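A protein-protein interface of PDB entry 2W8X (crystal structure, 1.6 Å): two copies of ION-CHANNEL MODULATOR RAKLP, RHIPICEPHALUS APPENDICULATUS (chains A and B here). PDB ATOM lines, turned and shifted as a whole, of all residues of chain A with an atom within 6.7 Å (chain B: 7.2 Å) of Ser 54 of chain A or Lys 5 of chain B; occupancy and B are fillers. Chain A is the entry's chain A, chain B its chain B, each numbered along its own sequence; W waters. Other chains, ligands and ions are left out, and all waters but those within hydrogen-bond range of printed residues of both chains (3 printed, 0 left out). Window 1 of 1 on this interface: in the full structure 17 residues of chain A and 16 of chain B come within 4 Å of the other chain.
Leu 31 of chain A touches Ser 54 of chain B, and with the chains exchanged Ser 54 of chain A touches Leu 31 of chain B. Ser 52 of chain A touches Ser 54 of chain B, and with the chains exchanged Ser 54 of chain A touches Ser 52 of chain B. Positions printed for both chains: 31, 52, 53 and 54.
NZ of Lys 5 of chain B is in hydrogen-bond range of OG of Ser 52 of chain B (3.0 Å). SG of Cys 50 of chain B is disulfide-bonded to SG of Cys 10 of chain B (2.1 Å). ND2 of Asn 2 of chain B is in hydrogen-bond range of O of Gly 8 of chain B (3.2 Å). O of Leu 24 of chain B lies within hydrogen-bond range of N of Asp 48 of chain B, at 2.9 Å. The side-chain amide nitrogen (ND2) of Asn 4 of chain B sits at hydrogen-bond distance from the side-chain carboxylate (OE2) of Glu 7 of chain B (3.3 Å). The side-chain hydroxyl (OG) of Ser 55 of chain A lies within hydrogen-bond range of the backbone NH (N) of Ala 58 of chain A.
Printed residues of chain A that touch a printed residue of chain B: Leu 31, Ser 52, Ser 54, Ser 55, Gly 57, Ala 58 and Met 61. Hydrophobic or aromatic side chains of chain A that line the printed part of chain B: Leu 31, Ala 58 and Met 61. Of the 23 printed residues of chain B, 9 touch a printed residue of chain A. Hydrophobic or aromatic side chains of chain B within 4 Å of the printed part of chain A: Leu 31. Among the printed residues, 15 pairs touch across the chains. Among the printed residues, no Asp or Glu carboxylate lies within 4 Å of a Lys or Arg side-chain nitrogen of the other chain.
Water W2 lies within hydrogen-bond range of NH1 of Arg 6 of chain B (2.8 Å), OD1 of Asp 48 of chain B (3.0 Å), N of Gly 57 of chain A (3.1 Å) and OG of Ser 55 of chain A (3.2 Å). Water W1 bridges O of Gly 57 of chain A (2.9 Å) and O of Arg 6 of chain B (3.1 Å). Water W3 bridges NZ of Lys 5 of chain B (2.9 Å) and N of Ser 54 of chain A (3.0 Å).
Among the printed residues, merely in contact across the chains: Met 61 of chain A with Arg 6 of chain B (3.1 Å), Met 61 of chain A with Lys 5 of chain B (3.4 Å), Gly 57 of chain A with Arg 6 of chain B (3.5 Å), Ala 58 of chain A with Lys 5 of chain B (3.7 Å), Met 61 of chain A with Gly 8 of chain B (3.7 Å), Ser 55 of chain A with Arg 47 of chain B (3.7 Å), Ser 52 of chain A with Ser 54 of chain B (3.7 Å), Ser 54 of chain A with Ser 52 of chain B (3.8 Å), Met 61 of chain A with Glu 7 of chain B (3.9 Å), Leu 31 of chain A with Ser 54 of chain B (3.9 Å), Gly 57 of chain A with Lys 5 of chain B (3.9 Å) and Ser 54 of chain A with Leu 31 of chain B (3.98 Å).
The side-chain hydroxyl of Ser 54 of chain A lies within hydrogen-bond range of the backbone carbonyl oxygen of Arg 47 of chain B, at 2.6 Å. The side-chain hydroxyl (OG) of Ser 54 of chain A is in hydrogen-bond range of the side-chain amino group (NZ) of Lys 5 of chain B, 2.9 Å away. The side-chain hydroxyl (OG) of Ser 55 of chain A lies within hydrogen-bond range of the side-chain carboxylate (OD1) of Asp 48 of chain B (2.7 Å).
Printed residues of chain B within 4 Å of Ser 54 of chain A: Lys 5 (2.9 Å), Leu 31 (3.98 Å), Arg 47 (2.6 Å) and Ser 52 (3.8 Å). Of the printed residues of chain A, Lys 5 of chain B touches Ser 54, Gly 57, Ala 58 and Met 61. Of the printed residues of chain A, Arg 6 of chain B touches Gly 57 (3.5 Å) and Met 61 (3.1 Å). Of the printed residues of chain B, Leu 31 of chain A touches Ser 54. Of the printed residues of chain A, Ser 52 of chain B touches Ser 54. Of the printed residues of chain B, Met 61 of chain A touches Lys 5, Arg 6, Glu 7 and Gly 8.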
ATOM      1  N   GLN A  30     -32.528 -21.803  -9.899  1.00  0.00           N
ATOM      2  CA  GLN A  30     -31.982 -22.515  -8.745  1.00  0.00           C
ATOM      3  C   GLN A  30     -31.721 -21.639  -7.524  1.00  0.00           C
ATOM      4  O   GLN A  30     -31.378 -22.152  -6.447  1.00  0.00           O
ATOM      5  CB  GLN A  30     -30.700 -23.256  -9.125  1.00  0.00           C
ATOM      6  CG  GLN A  30     -30.923 -24.507  -9.985  1.00  0.00           C
ATOM      7  CD  GLN A  30     -31.473 -24.276 -11.368  1.00  0.00           C
ATOM      8  OE1 GLN A  30     -32.434 -24.949 -11.769  1.00  0.00           O
ATOM      9  NE2 GLN A  30     -30.874 -23.361 -12.116  1.00  0.00           N
ATOM     10  N   LEU A  31     -31.871 -20.323  -7.684  1.00  0.00           N
ATOM     11  CA  LEU A  31     -31.829 -19.423  -6.538  1.00  0.00           C
ATOM     12  C   LEU A  31     -33.199 -19.429  -5.858  1.00  0.00           C
ATOM     13  O   LEU A  31     -34.151 -19.956  -6.401  1.00  0.00           O
ATOM     14  CB  LEU A  31     -31.402 -18.017  -6.966  1.00  0.00           C
ATOM     15  CG  LEU A  31     -29.989 -17.938  -7.543  1.00  0.00           C
ATOM     16  CD1 LEU A  31     -29.701 -16.485  -7.909  1.00  0.00           C
ATOM     17  CD2 LEU A  31     -28.901 -18.495  -6.593  1.00  0.00           C
ATOM     18  N   TRP A  32     -33.267 -18.828  -4.670  1.00  0.00           N
ATOM     19  CA  TRP A  32     -34.492 -18.634  -3.912  1.00  0.00           C
ATOM     20  C   TRP A  32     -34.676 -17.159  -3.556  1.00  0.00           C
ATOM     21  O   TRP A  32     -33.717 -16.371  -3.573  1.00  0.00           O
ATOM     22  CB  TRP A  32     -34.387 -19.456  -2.605  1.00  0.00           C
ATOM     23  CG  TRP A  32     -34.339 -20.945  -2.869  1.00  0.00           C
ATOM     24  CD1 TRP A  32     -33.298 -21.660  -3.393  1.00  0.00           C
ATOM     25  CD2 TRP A  32     -35.409 -21.888  -2.667  1.00  0.00           C
ATOM     26  NE1 TRP A  32     -33.651 -22.988  -3.532  1.00  0.00           N
ATOM     27  CE2 TRP A  32     -34.937 -23.154  -3.086  1.00  0.00           C
ATOM     28  CE3 TRP A  32     -36.701 -21.787  -2.152  1.00  0.00           C
ATOM     29  CZ2 TRP A  32     -35.729 -24.296  -2.988  1.00  0.00           C
ATOM     30  CZ3 TRP A  32     -37.475 -22.924  -2.061  1.00  0.00           C
ATOM     31  CH2 TRP A  32     -36.985 -24.146  -2.491  1.00  0.00           C
ATOM     32  N   SER A  52     -31.916 -12.517  -3.099  1.00  0.00           N
ATOM     33  CA  SER A  52     -31.685 -13.758  -3.878  1.00  0.00           C
ATOM     34  C   SER A  52     -30.735 -14.574  -3.039  1.00  0.00           C
ATOM     35  O   SER A  52     -29.773 -14.028  -2.468  1.00  0.00           O
ATOM     36  CB  SER A  52     -31.096 -13.509  -5.290  1.00  0.00           C
ATOM     37  OG  SER A  52     -29.818 -12.912  -5.262  1.00  0.00           O
ATOM     38  N   HIS A  53     -31.050 -15.848  -2.904  1.00  0.00           N
ATOM     39  CA  HIS A  53     -30.418 -16.722  -1.904  1.00  0.00           C
ATOM     40  C   HIS A  53     -29.968 -18.016  -2.554  1.00  0.00           C
ATOM     41  O   HIS A  53     -30.626 -18.520  -3.458  1.00  0.00           O
ATOM     42  CB  HIS A  53     -31.415 -16.998  -0.782  1.00  0.00           C
ATOM     43  CG  HIS A  53     -31.923 -15.750  -0.133  1.00  0.00           C
ATOM     44  ND1 HIS A  53     -31.440 -15.287   1.079  1.00  0.00           N
ATOM     45  CD2 HIS A  53     -32.871 -14.869  -0.528  1.00  0.00           C
ATOM     46  CE1 HIS A  53     -32.083 -14.175   1.391  1.00  0.00           C
ATOM     47  NE2 HIS A  53     -32.940 -13.886   0.422  1.00  0.00           N
ATOM     48  N   SER A  54     -28.836 -18.553  -2.096  1.00  0.00           N
ATOM     49  CA  SER A  54     -28.237 -19.727  -2.725  1.00  0.00           C
ATOM     50  C   SER A  54     -28.903 -21.065  -2.422  1.00  0.00           C
ATOM     51  O   SER A  54     -28.668 -22.052  -3.120  1.00  0.00           O
ATOM     52  CB  SER A  54     -26.766 -19.789  -2.366  1.00  0.00           C
ATOM     53  OG  SER A  54     -26.554 -19.824  -0.966  1.00  0.00           O
ATOM     54  N   SER A  55     -29.717 -21.098  -1.376  1.00  0.00           N
ATOM     55  CA  SER A  55     -30.479 -22.299  -1.010  1.00  0.00           C
ATOM     56  C   SER A  55     -31.723 -21.923  -0.228  1.00  0.00           C
ATOM     57  O   SER A  55     -31.820 -20.824   0.306  1.00  0.00           O
ATOM     58  CB  SER A  55     -29.614 -23.222  -0.149  1.00  0.00           C
ATOM     59  OG  SER A  55     -29.360 -22.660   1.160  1.00  0.00           O
ATOM     60  N   SER A  56     -32.674 -22.857  -0.136  1.00  0.00           N
ATOM     61  CA  SER A  56     -33.868 -22.660   0.684  1.00  0.00           C
ATOM     62  C   SER A  56     -33.474 -22.462   2.141  1.00  0.00           C
ATOM     63  O   SER A  56     -34.004 -21.582   2.808  1.00  0.00           O
ATOM     64  CB  SER A  56     -34.883 -23.812   0.523  1.00  0.00           C
ATOM     65  OG  SER A  56     -36.016 -23.664   1.391  1.00  0.00           O
ATOM     66  N   GLY A  57     -32.527 -23.253   2.632  1.00  0.00           N
ATOM     67  CA  GLY A  57     -32.105 -23.108   4.015  1.00  0.00           C
ATOM     68  C   GLY A  57     -31.475 -21.785   4.369  1.00  0.00           C
ATOM     69  O   GLY A  57     -31.682 -21.255   5.471  1.00  0.00           O
ATOM     70  N   ALA A  58     -30.704 -21.235   3.435  1.00  0.00           N
ATOM     71  CA  ALA A  58     -30.103 -19.908   3.597  1.00  0.00           C
ATOM     72  C   ALA A  58     -31.200 -18.846   3.714  1.00  0.00           C
ATOM     73  O   ALA A  58     -31.145 -17.971   4.582  1.00  0.00           O
ATOM     74  CB  ALA A  58     -29.191 -19.609   2.404  1.00  0.00           C
ATOM     75  N   CYS A  59     -32.194 -18.933   2.832  1.00  0.00           N
ATOM     76  CA  CYS A  59     -33.302 -17.998   2.836  1.00  0.00           C
ATOM     77  C   CYS A  59     -34.129 -18.116   4.117  1.00  0.00           C
ATOM     78  O   CYS A  59     -34.517 -17.104   4.743  1.00  0.00           O
ATOM     79  CB  CYS A  59     -34.151 -18.193   1.559  1.00  0.00           C
ATOM     80  SG  CYS A  59     -35.542 -17.058   1.445  1.00  0.00           S
ATOM     81  N   VAL A  60     -34.396 -19.353   4.520  1.00  0.00           N
ATOM     82  CA  VAL A  60     -35.186 -19.606   5.708  1.00  0.00           C
ATOM     83  C   VAL A  60     -34.505 -18.984   6.928  1.00  0.00           C
ATOM     84  O   VAL A  60     -35.140 -18.266   7.706  1.00  0.00           O
ATOM     85  CB  VAL A  60     -35.484 -21.100   5.884  1.00  0.00           C
ATOM     86  CG1 VAL A  60     -36.012 -21.365   7.300  1.00  0.00           C
ATOM     87  CG2 VAL A  60     -36.467 -21.535   4.799  1.00  0.00           C
ATOM     88  N   MET A  61     -33.222 -19.255   7.099  1.00  0.00           N
ATOM     89  CA  MET A  61     -32.492 -18.693   8.218  1.00  0.00           C
ATOM     90  C   MET A  61     -32.422 -17.173   8.194  1.00  0.00           C
ATOM     91  O   MET A  61     -32.751 -16.519   9.192  1.00  0.00           O
ATOM     92  CB  MET A  61     -31.080 -19.275   8.302  1.00  0.00           C
ATOM     93  CG  MET A  61     -30.227 -18.688   9.414  1.00  0.00           C
ATOM     94  SD  MET A  61     -30.922 -18.824  11.063  1.00  0.00           S
ATOM     95  CE  MET A  61     -31.032 -20.578  11.190  1.00  0.00           C
ATOM     96  N   ALA A  62     -32.019 -16.589   7.073  1.00  0.00           N
ATOM     97  CA  ALA A  62     -31.866 -15.145   7.026  1.00  0.00           C
ATOM     98  C   ALA A  62     -33.183 -14.399   7.181  1.00  0.00           C
ATOM     99  O   ALA A  62     -33.215 -13.307   7.767  1.00  0.00           O
ATOM    100  CB  ALA A  62     -31.185 -14.710   5.733  1.00  0.00           C
ATOM    101  N   ASN B   2     -19.602 -17.374  12.027  1.00  0.00           N
ATOM    102  CA  ASN B   2     -20.410 -18.410  11.382  1.00  0.00           C
ATOM    103  C   ASN B   2     -20.112 -18.502   9.892  1.00  0.00           C
ATOM    104  O   ASN B   2     -20.047 -17.460   9.237  1.00  0.00           O
ATOM    105  CB  ASN B   2     -21.890 -18.100  11.533  1.00  0.00           C
ATOM    106  CG  ASN B   2     -22.789 -19.116  10.827  1.00  0.00           C
ATOM    107  OD1 ASN B   2     -22.642 -20.326  11.000  1.00  0.00           O
ATOM    108  ND2 ASN B   2     -23.711 -18.618  10.003  1.00  0.00           N
ATOM    109  N   CYS B   3     -19.993 -19.732   9.382  1.00  0.00           N
ATOM    110  CA  CYS B   3     -19.834 -19.966   7.943  1.00  0.00           C
ATOM    111  C   CYS B   3     -20.943 -20.787   7.303  1.00  0.00           C
ATOM    112  O   CYS B   3     -20.893 -21.017   6.087  1.00  0.00           O
ATOM    113  CB  CYS B   3     -18.476 -20.609   7.615  1.00  0.00           C
ATOM    114  SG  CYS B   3     -17.082 -19.447   7.920  1.00  0.00           S
ATOM    115  N   ASN B   4     -21.952 -21.199   8.074  1.00  0.00           N
ATOM    116  CA  ASN B   4     -23.031 -22.010   7.533  1.00  0.00           C
ATOM    117  C   ASN B   4     -24.326 -21.191   7.454  1.00  0.00           C
ATOM    118  O   ASN B   4     -24.879 -20.786   8.474  1.00  0.00           O
ATOM    119  CB  ASN B   4     -23.233 -23.260   8.391  1.00  0.00           C
ATOM    120  CG  ASN B   4     -24.169 -24.246   7.778  1.00  0.00           C
ATOM    121  OD1 ASN B   4     -25.148 -23.892   7.114  1.00  0.00           O
ATOM    122  ND2 ASN B   4     -23.897 -25.519   8.021  1.00  0.00           N
ATOM    123  N   LYS B   5     -24.785 -20.938   6.228  1.00  0.00           N
ATOM    124  CA  LYS B   5     -25.956 -20.115   5.962  1.00  0.00           C
ATOM    125  C   LYS B   5     -27.225 -20.672   6.539  1.00  0.00           C
ATOM    126  O   LYS B   5     -28.189 -19.911   6.724  1.00  0.00           O
ATOM    127  CB  LYS B   5     -26.168 -19.972   4.438  1.00  0.00           C
ATOM    128  CG  LYS B   5     -25.154 -19.166   3.747  1.00  0.00           C
ATOM    129  CD  LYS B   5     -25.429 -19.071   2.229  1.00  0.00           C
ATOM    130  CE  LYS B   5     -24.595 -18.031   1.587  1.00  0.00           C
ATOM    131  NZ  LYS B   5     -24.781 -17.895   0.170  1.00  0.00           N
ATOM    132  N   ARG B   6     -27.249 -21.983   6.771  1.00  0.00           N
ATOM    133  CA  ARG B   6     -28.410 -22.649   7.383  1.00  0.00           C
ATOM    134  C   ARG B   6     -28.490 -22.457   8.859  1.00  0.00           C
ATOM    135  O   ARG B   6     -29.578 -22.662   9.439  1.00  0.00           O
ATOM    136  CB  ARG B   6     -28.356 -24.160   7.191  1.00  0.00           C
ATOM    137  CG  ARG B   6     -28.638 -24.576   5.825  1.00  0.00           C
ATOM    138  CD  ARG B   6     -28.697 -26.114   5.708  1.00  0.00           C
ATOM    139  NE  ARG B   6     -29.803 -26.679   6.478  1.00  0.00           N
ATOM    140  CZ  ARG B   6     -31.068 -26.818   6.061  1.00  0.00           C
ATOM    141  NH1 ARG B   6     -31.466 -26.435   4.849  1.00  0.00           N
ATOM    142  NH2 ARG B   6     -31.962 -27.349   6.893  1.00  0.00           N
ATOM    143  N   GLU B   7     -27.360 -22.128   9.479  1.00  0.00           N
ATOM    144  CA  GLU B   7     -27.226 -22.157  10.946  1.00  0.00           C
ATOM    145  C   GLU B   7     -27.147 -20.781  11.619  1.00  0.00           C
ATOM    146  O   GLU B   7     -27.259 -20.671  12.845  1.00  0.00           O
ATOM    147  CB  GLU B   7     -26.002 -23.005  11.312  1.00  0.00           C
ATOM    148  CG  GLU B   7     -26.119 -24.432  10.881  1.00  0.00           C
ATOM    149  CD  GLU B   7     -24.903 -25.283  11.271  1.00  0.00           C
ATOM    150  OE1 GLU B   7     -23.935 -24.743  11.878  1.00  0.00           O
ATOM    151  OE2 GLU B   7     -24.932 -26.505  10.962  1.00  0.00           O
ATOM    152  N   GLY B   8     -26.947 -19.730  10.851  1.00  0.00           N
ATOM    153  CA  GLY B   8     -26.885 -18.376  11.371  1.00  0.00           C
ATOM    154  C   GLY B   8     -26.681 -17.368  10.253  1.00  0.00           C
ATOM    155  O   GLY B   8     -26.659 -17.774   9.100  1.00  0.00           O
ATOM    156  N   PRO B   9     -26.480 -16.078  10.591  1.00  0.00           N
ATOM    157  CA  PRO B   9     -26.316 -15.031   9.606  1.00  0.00           C
ATOM    158  C   PRO B   9     -24.922 -15.078   9.015  1.00  0.00           C
ATOM    159  O   PRO B   9     -24.024 -15.681   9.603  1.00  0.00           O
ATOM    160  CB  PRO B   9     -26.480 -13.755  10.424  1.00  0.00           C
ATOM    161  CG  PRO B   9     -25.958 -14.136  11.716  1.00  0.00           C
ATOM    162  CD  PRO B   9     -26.345 -15.534  11.953  1.00  0.00           C
ATOM    163  N   CYS B  10     -24.758 -14.459   7.859  1.00  0.00           N
ATOM    164  CA  CYS B  10     -23.453 -14.287   7.268  1.00  0.00           C
ATOM    165  C   CYS B  10     -23.053 -12.835   7.342  1.00  0.00           C
ATOM    166  O   CYS B  10     -23.626 -11.998   6.651  1.00  0.00           O
ATOM    167  CB  CYS B  10     -23.465 -14.747   5.815  1.00  0.00           C
ATOM    168  SG  CYS B  10     -23.748 -16.513   5.586  1.00  0.00           S
ATOM    169  N   LEU B  15     -18.578 -13.538   4.257  1.00  0.00           N
ATOM    170  CA  LEU B  15     -18.745 -13.643   2.809  1.00  0.00           C
ATOM    171  C   LEU B  15     -17.434 -13.818   2.077  1.00  0.00           C
ATOM    172  O   LEU B  15     -17.378 -14.465   1.004  1.00  0.00           O
ATOM    173  CB  LEU B  15     -19.412 -12.381   2.227  1.00  0.00           C
ATOM    174  CG  LEU B  15     -20.788 -11.971   2.708  1.00  0.00           C
ATOM    175  CD1 LEU B  15     -21.357 -10.838   1.825  1.00  0.00           C
ATOM    176  CD2 LEU B  15     -21.752 -13.147   2.849  1.00  0.00           C
ATOM    177  N   LEU B  24     -20.477 -27.376   2.539  1.00  0.00           N
ATOM    178  CA  LEU B  24     -21.699 -27.093   3.276  1.00  0.00           C
ATOM    179  C   LEU B  24     -22.794 -26.944   2.243  1.00  0.00           C
ATOM    180  O   LEU B  24     -22.861 -25.937   1.515  1.00  0.00           O
ATOM    181  CB  LEU B  24     -21.537 -25.835   4.110  1.00  0.00           C
ATOM    182  CG  LEU B  24     -20.375 -25.788   5.095  1.00  0.00           C
ATOM    183  CD1 LEU B  24     -20.223 -24.430   5.734  1.00  0.00           C
ATOM    184  CD2 LEU B  24     -20.506 -26.860   6.153  1.00  0.00           C
ATOM    185  N   ARG B  26     -24.962 -28.607  -1.180  1.00  0.00           N
ATOM    186  CA  ARG B  26     -24.597 -29.025  -2.505  1.00  0.00           C
ATOM    187  C   ARG B  26     -23.738 -27.994  -3.227  1.00  0.00           C
ATOM    188  O   ARG B  26     -23.948 -26.775  -3.105  1.00  0.00           O
ATOM    189  CB  ARG B  26     -25.862 -29.249  -3.301  1.00  0.00           C
ATOM    190  CG  ARG B  26     -25.702 -29.766  -4.689  1.00  0.00           C
ATOM    191  CD  ARG B  26     -27.054 -30.130  -5.283  1.00  0.00           C
ATOM    192  NE  ARG B  26     -27.830 -31.057  -4.429  1.00  0.00           N
ATOM    193  CZ  ARG B  26     -27.692 -32.387  -4.378  1.00  0.00           C
ATOM    194  NH1 ARG B  26     -26.786 -33.024  -5.120  1.00  0.00           N
ATOM    195  NH2 ARG B  26     -28.467 -33.094  -3.570  1.00  0.00           N
ATOM    196  N   SER B  28     -22.522 -25.979  -6.526  1.00  0.00           N
ATOM    197  CA  SER B  28     -23.057 -25.462  -7.792  1.00  0.00           C
ATOM    198  C   SER B  28     -22.003 -24.728  -8.583  1.00  0.00           C
ATOM    199  O   SER B  28     -21.304 -23.874  -8.044  1.00  0.00           O
ATOM    200  CB  SER B  28     -24.217 -24.503  -7.532  1.00  0.00           C
ATOM    201  OG  SER B  28     -24.639 -23.824  -8.701  1.00  0.00           O
ATOM    202  N   LEU B  31     -22.704 -20.794  -8.906  1.00  0.00           N
ATOM    203  CA  LEU B  31     -22.333 -19.882  -7.833  1.00  0.00           C
ATOM    204  C   LEU B  31     -20.854 -19.527  -7.965  1.00  0.00           C
ATOM    205  O   LEU B  31     -20.137 -20.168  -8.742  1.00  0.00           O
ATOM    206  CB  LEU B  31     -22.629 -20.496  -6.486  1.00  0.00           C
ATOM    207  CG  LEU B  31     -24.062 -20.934  -6.218  1.00  0.00           C
ATOM    208  CD1 LEU B  31     -24.194 -21.585  -4.820  1.00  0.00           C
ATOM    209  CD2 LEU B  31     -25.028 -19.732  -6.369  1.00  0.00           C
ATOM    210  N   TYR B  46     -20.354 -23.849  -2.599  1.00  0.00           N
ATOM    211  CA  TYR B  46     -21.200 -24.722  -1.797  1.00  0.00           C
ATOM    212  C   TYR B  46     -22.340 -23.878  -1.249  1.00  0.00           C
ATOM    213  O   TYR B  46     -22.122 -22.865  -0.590  1.00  0.00           O
ATOM    214  CB  TYR B  46     -20.377 -25.416  -0.693  1.00  0.00           C
ATOM    215  CG  TYR B  46     -19.406 -26.396  -1.250  1.00  0.00           C
ATOM    216  CD1 TYR B  46     -19.834 -27.670  -1.647  1.00  0.00           C
ATOM    217  CD2 TYR B  46     -18.062 -26.077  -1.392  1.00  0.00           C
ATOM    218  CE1 TYR B  46     -18.935 -28.570  -2.147  1.00  0.00           C
ATOM    219  CE2 TYR B  46     -17.171 -26.969  -1.901  1.00  0.00           C
ATOM    220  CZ  TYR B  46     -17.609 -28.204  -2.295  1.00  0.00           C
ATOM    221  OH  TYR B  46     -16.662 -29.091  -2.802  1.00  0.00           O
ATOM    222  N   ARG B  47     -23.567 -24.304  -1.509  1.00  0.00           N
ATOM    223  CA  ARG B  47     -24.714 -23.403  -1.399  1.00  0.00           C
ATOM    224  C   ARG B  47     -25.081 -22.985   0.017  1.00  0.00           C
ATOM    225  O   ARG B  47     -25.834 -22.030   0.195  1.00  0.00           O
ATOM    226  CB  ARG B  47     -25.918 -23.975  -2.102  1.00  0.00           C
ATOM    227  CG  ARG B  47     -26.497 -25.150  -1.438  1.00  0.00           C
ATOM    228  CD  ARG B  47     -27.527 -25.750  -2.265  1.00  0.00           C
ATOM    229  NE  ARG B  47     -28.170 -26.875  -1.621  1.00  0.00           N
ATOM    230  CZ  ARG B  47     -28.941 -27.769  -2.258  1.00  0.00           C
ATOM    231  NH1 ARG B  47     -29.112 -27.728  -3.563  1.00  0.00           N
ATOM    232  NH2 ARG B  47     -29.453 -28.776  -1.560  1.00  0.00           N
ATOM    233  N   ASP B  48     -24.588 -23.716   1.030  1.00  0.00           N
ATOM    234  CA  ASP B  48     -24.796 -23.296   2.430  1.00  0.00           C
ATOM    235  C   ASP B  48     -23.566 -22.662   3.057  1.00  0.00           C
ATOM    236  O   ASP B  48     -23.550 -22.377   4.256  1.00  0.00           O
ATOM    237  CB  ASP B  48     -25.287 -24.457   3.305  1.00  0.00           C
ATOM    238  CG  ASP B  48     -26.626 -24.990   2.885  1.00  0.00           C
ATOM    239  OD1 ASP B  48     -27.466 -24.206   2.390  1.00  0.00           O
ATOM    240  OD2 ASP B  48     -26.840 -26.230   3.053  1.00  0.00           O
ATOM    241  N   ASN B  49     -22.529 -22.411   2.253  1.00  0.00           N
ATOM    242  CA  ASN B  49     -21.305 -21.767   2.745  1.00  0.00           C
ATOM    243  C   ASN B  49     -21.490 -20.247   2.625  1.00  0.00           C
ATOM    244  O   ASN B  49     -21.871 -19.755   1.564  1.00  0.00           O
ATOM    245  CB  ASN B  49     -20.145 -22.270   1.896  1.00  0.00           C
ATOM    246  CG  ASN B  49     -18.762 -21.805   2.369  1.00  0.00           C
ATOM    247  OD1 ASN B  49     -18.543 -20.645   2.793  1.00  0.00           O
ATOM    248  ND2 ASN B  49     -17.797 -22.738   2.305  1.00  0.00           N
ATOM    249  N   CYS B  50     -21.180 -19.492   3.670  1.00  0.00           N
ATOM    250  CA  CYS B  50     -21.311 -18.032   3.603  1.00  0.00           C
ATOM    251  C   CYS B  50     -20.513 -17.445   2.427  1.00  0.00           C
ATOM    252  O   CYS B  50     -20.902 -16.437   1.829  1.00  0.00           O
ATOM    253  CB  CYS B  50     -20.886 -17.345   4.928  1.00  0.00           C
ATOM    254  SG  CYS B  50     -22.083 -17.506   6.263  1.00  0.00           S
ATOM    255  N   ASN B  51     -19.352 -18.031   2.137  1.00  0.00           N
ATOM    256  CA  ASN B  51     -18.562 -17.672   0.959  1.00  0.00           C
ATOM    257  C   ASN B  51     -19.064 -18.464  -0.260  1.00  0.00           C
ATOM    258  O   ASN B  51     -18.390 -19.340  -0.778  1.00  0.00           O
ATOM    259  CB  ASN B  51     -17.075 -17.852   1.208  1.00  0.00           C
ATOM    260  CG  ASN B  51     -16.198 -17.291   0.093  1.00  0.00           C
ATOM    261  OD1 ASN B  51     -16.666 -16.792  -0.967  1.00  0.00           O
ATOM    262  ND2 ASN B  51     -14.879 -17.395   0.313  1.00  0.00           N
ATOM    263  N   SER B  52     -20.287 -18.120  -0.673  1.00  0.00           N
ATOM    264  CA  SER B  52     -20.883 -18.558  -1.928  1.00  0.00           C
ATOM    265  C   SER B  52     -21.780 -17.400  -2.354  1.00  0.00           C
ATOM    266  O   SER B  52     -22.548 -16.848  -1.537  1.00  0.00           O
ATOM    267  CB  SER B  52     -21.657 -19.874  -1.801  1.00  0.00           C
ATOM    268  OG  SER B  52     -22.801 -19.773  -0.960  1.00  0.00           O
ATOM    269  N   HIS B  53     -21.671 -17.043  -3.628  1.00  0.00           N
ATOM    270  CA  HIS B  53     -22.245 -15.800  -4.151  1.00  0.00           C
ATOM    271  C   HIS B  53     -23.063 -16.098  -5.397  1.00  0.00           C
ATOM    272  O   HIS B  53     -22.703 -16.991  -6.186  1.00  0.00           O
ATOM    273  CB  HIS B  53     -21.113 -14.796  -4.462  1.00  0.00           C
ATOM    274  CG  HIS B  53     -20.236 -14.496  -3.287  1.00  0.00           C
ATOM    275  ND1 HIS B  53     -20.318 -13.310  -2.585  1.00  0.00           N
ATOM    276  CD2 HIS B  53     -19.247 -15.218  -2.701  1.00  0.00           C
ATOM    277  CE1 HIS B  53     -19.412 -13.329  -1.609  1.00  0.00           C
ATOM    278  NE2 HIS B  53     -18.766 -14.486  -1.647  1.00  0.00           N
ATOM    279  N   SER B  54     -24.155 -15.357  -5.579  1.00  0.00           N
ATOM    280  CA  SER B  54     -25.096 -15.627  -6.665  1.00  0.00           C
ATOM    281  C   SER B  54     -24.626 -15.195  -8.046  1.00  0.00           C
ATOM    282  O   SER B  54     -25.204 -15.615  -9.063  1.00  0.00           O
ATOM    283  CB  SER B  54     -26.429 -14.990  -6.355  1.00  0.00           C
ATOM    284  OG  SER B  54     -26.279 -13.597  -6.167  1.00  0.00           O
HETATM  285  O   HOH W   1     -32.186 -22.974   7.760  1.00  0.00           O
HETATM  286  O   HOH W   2     -30.201 -25.361   2.624  1.00  0.00           O
HETATM  287  O   HOH W   3     -27.487 -16.785  -0.144  1.00  0.00           O
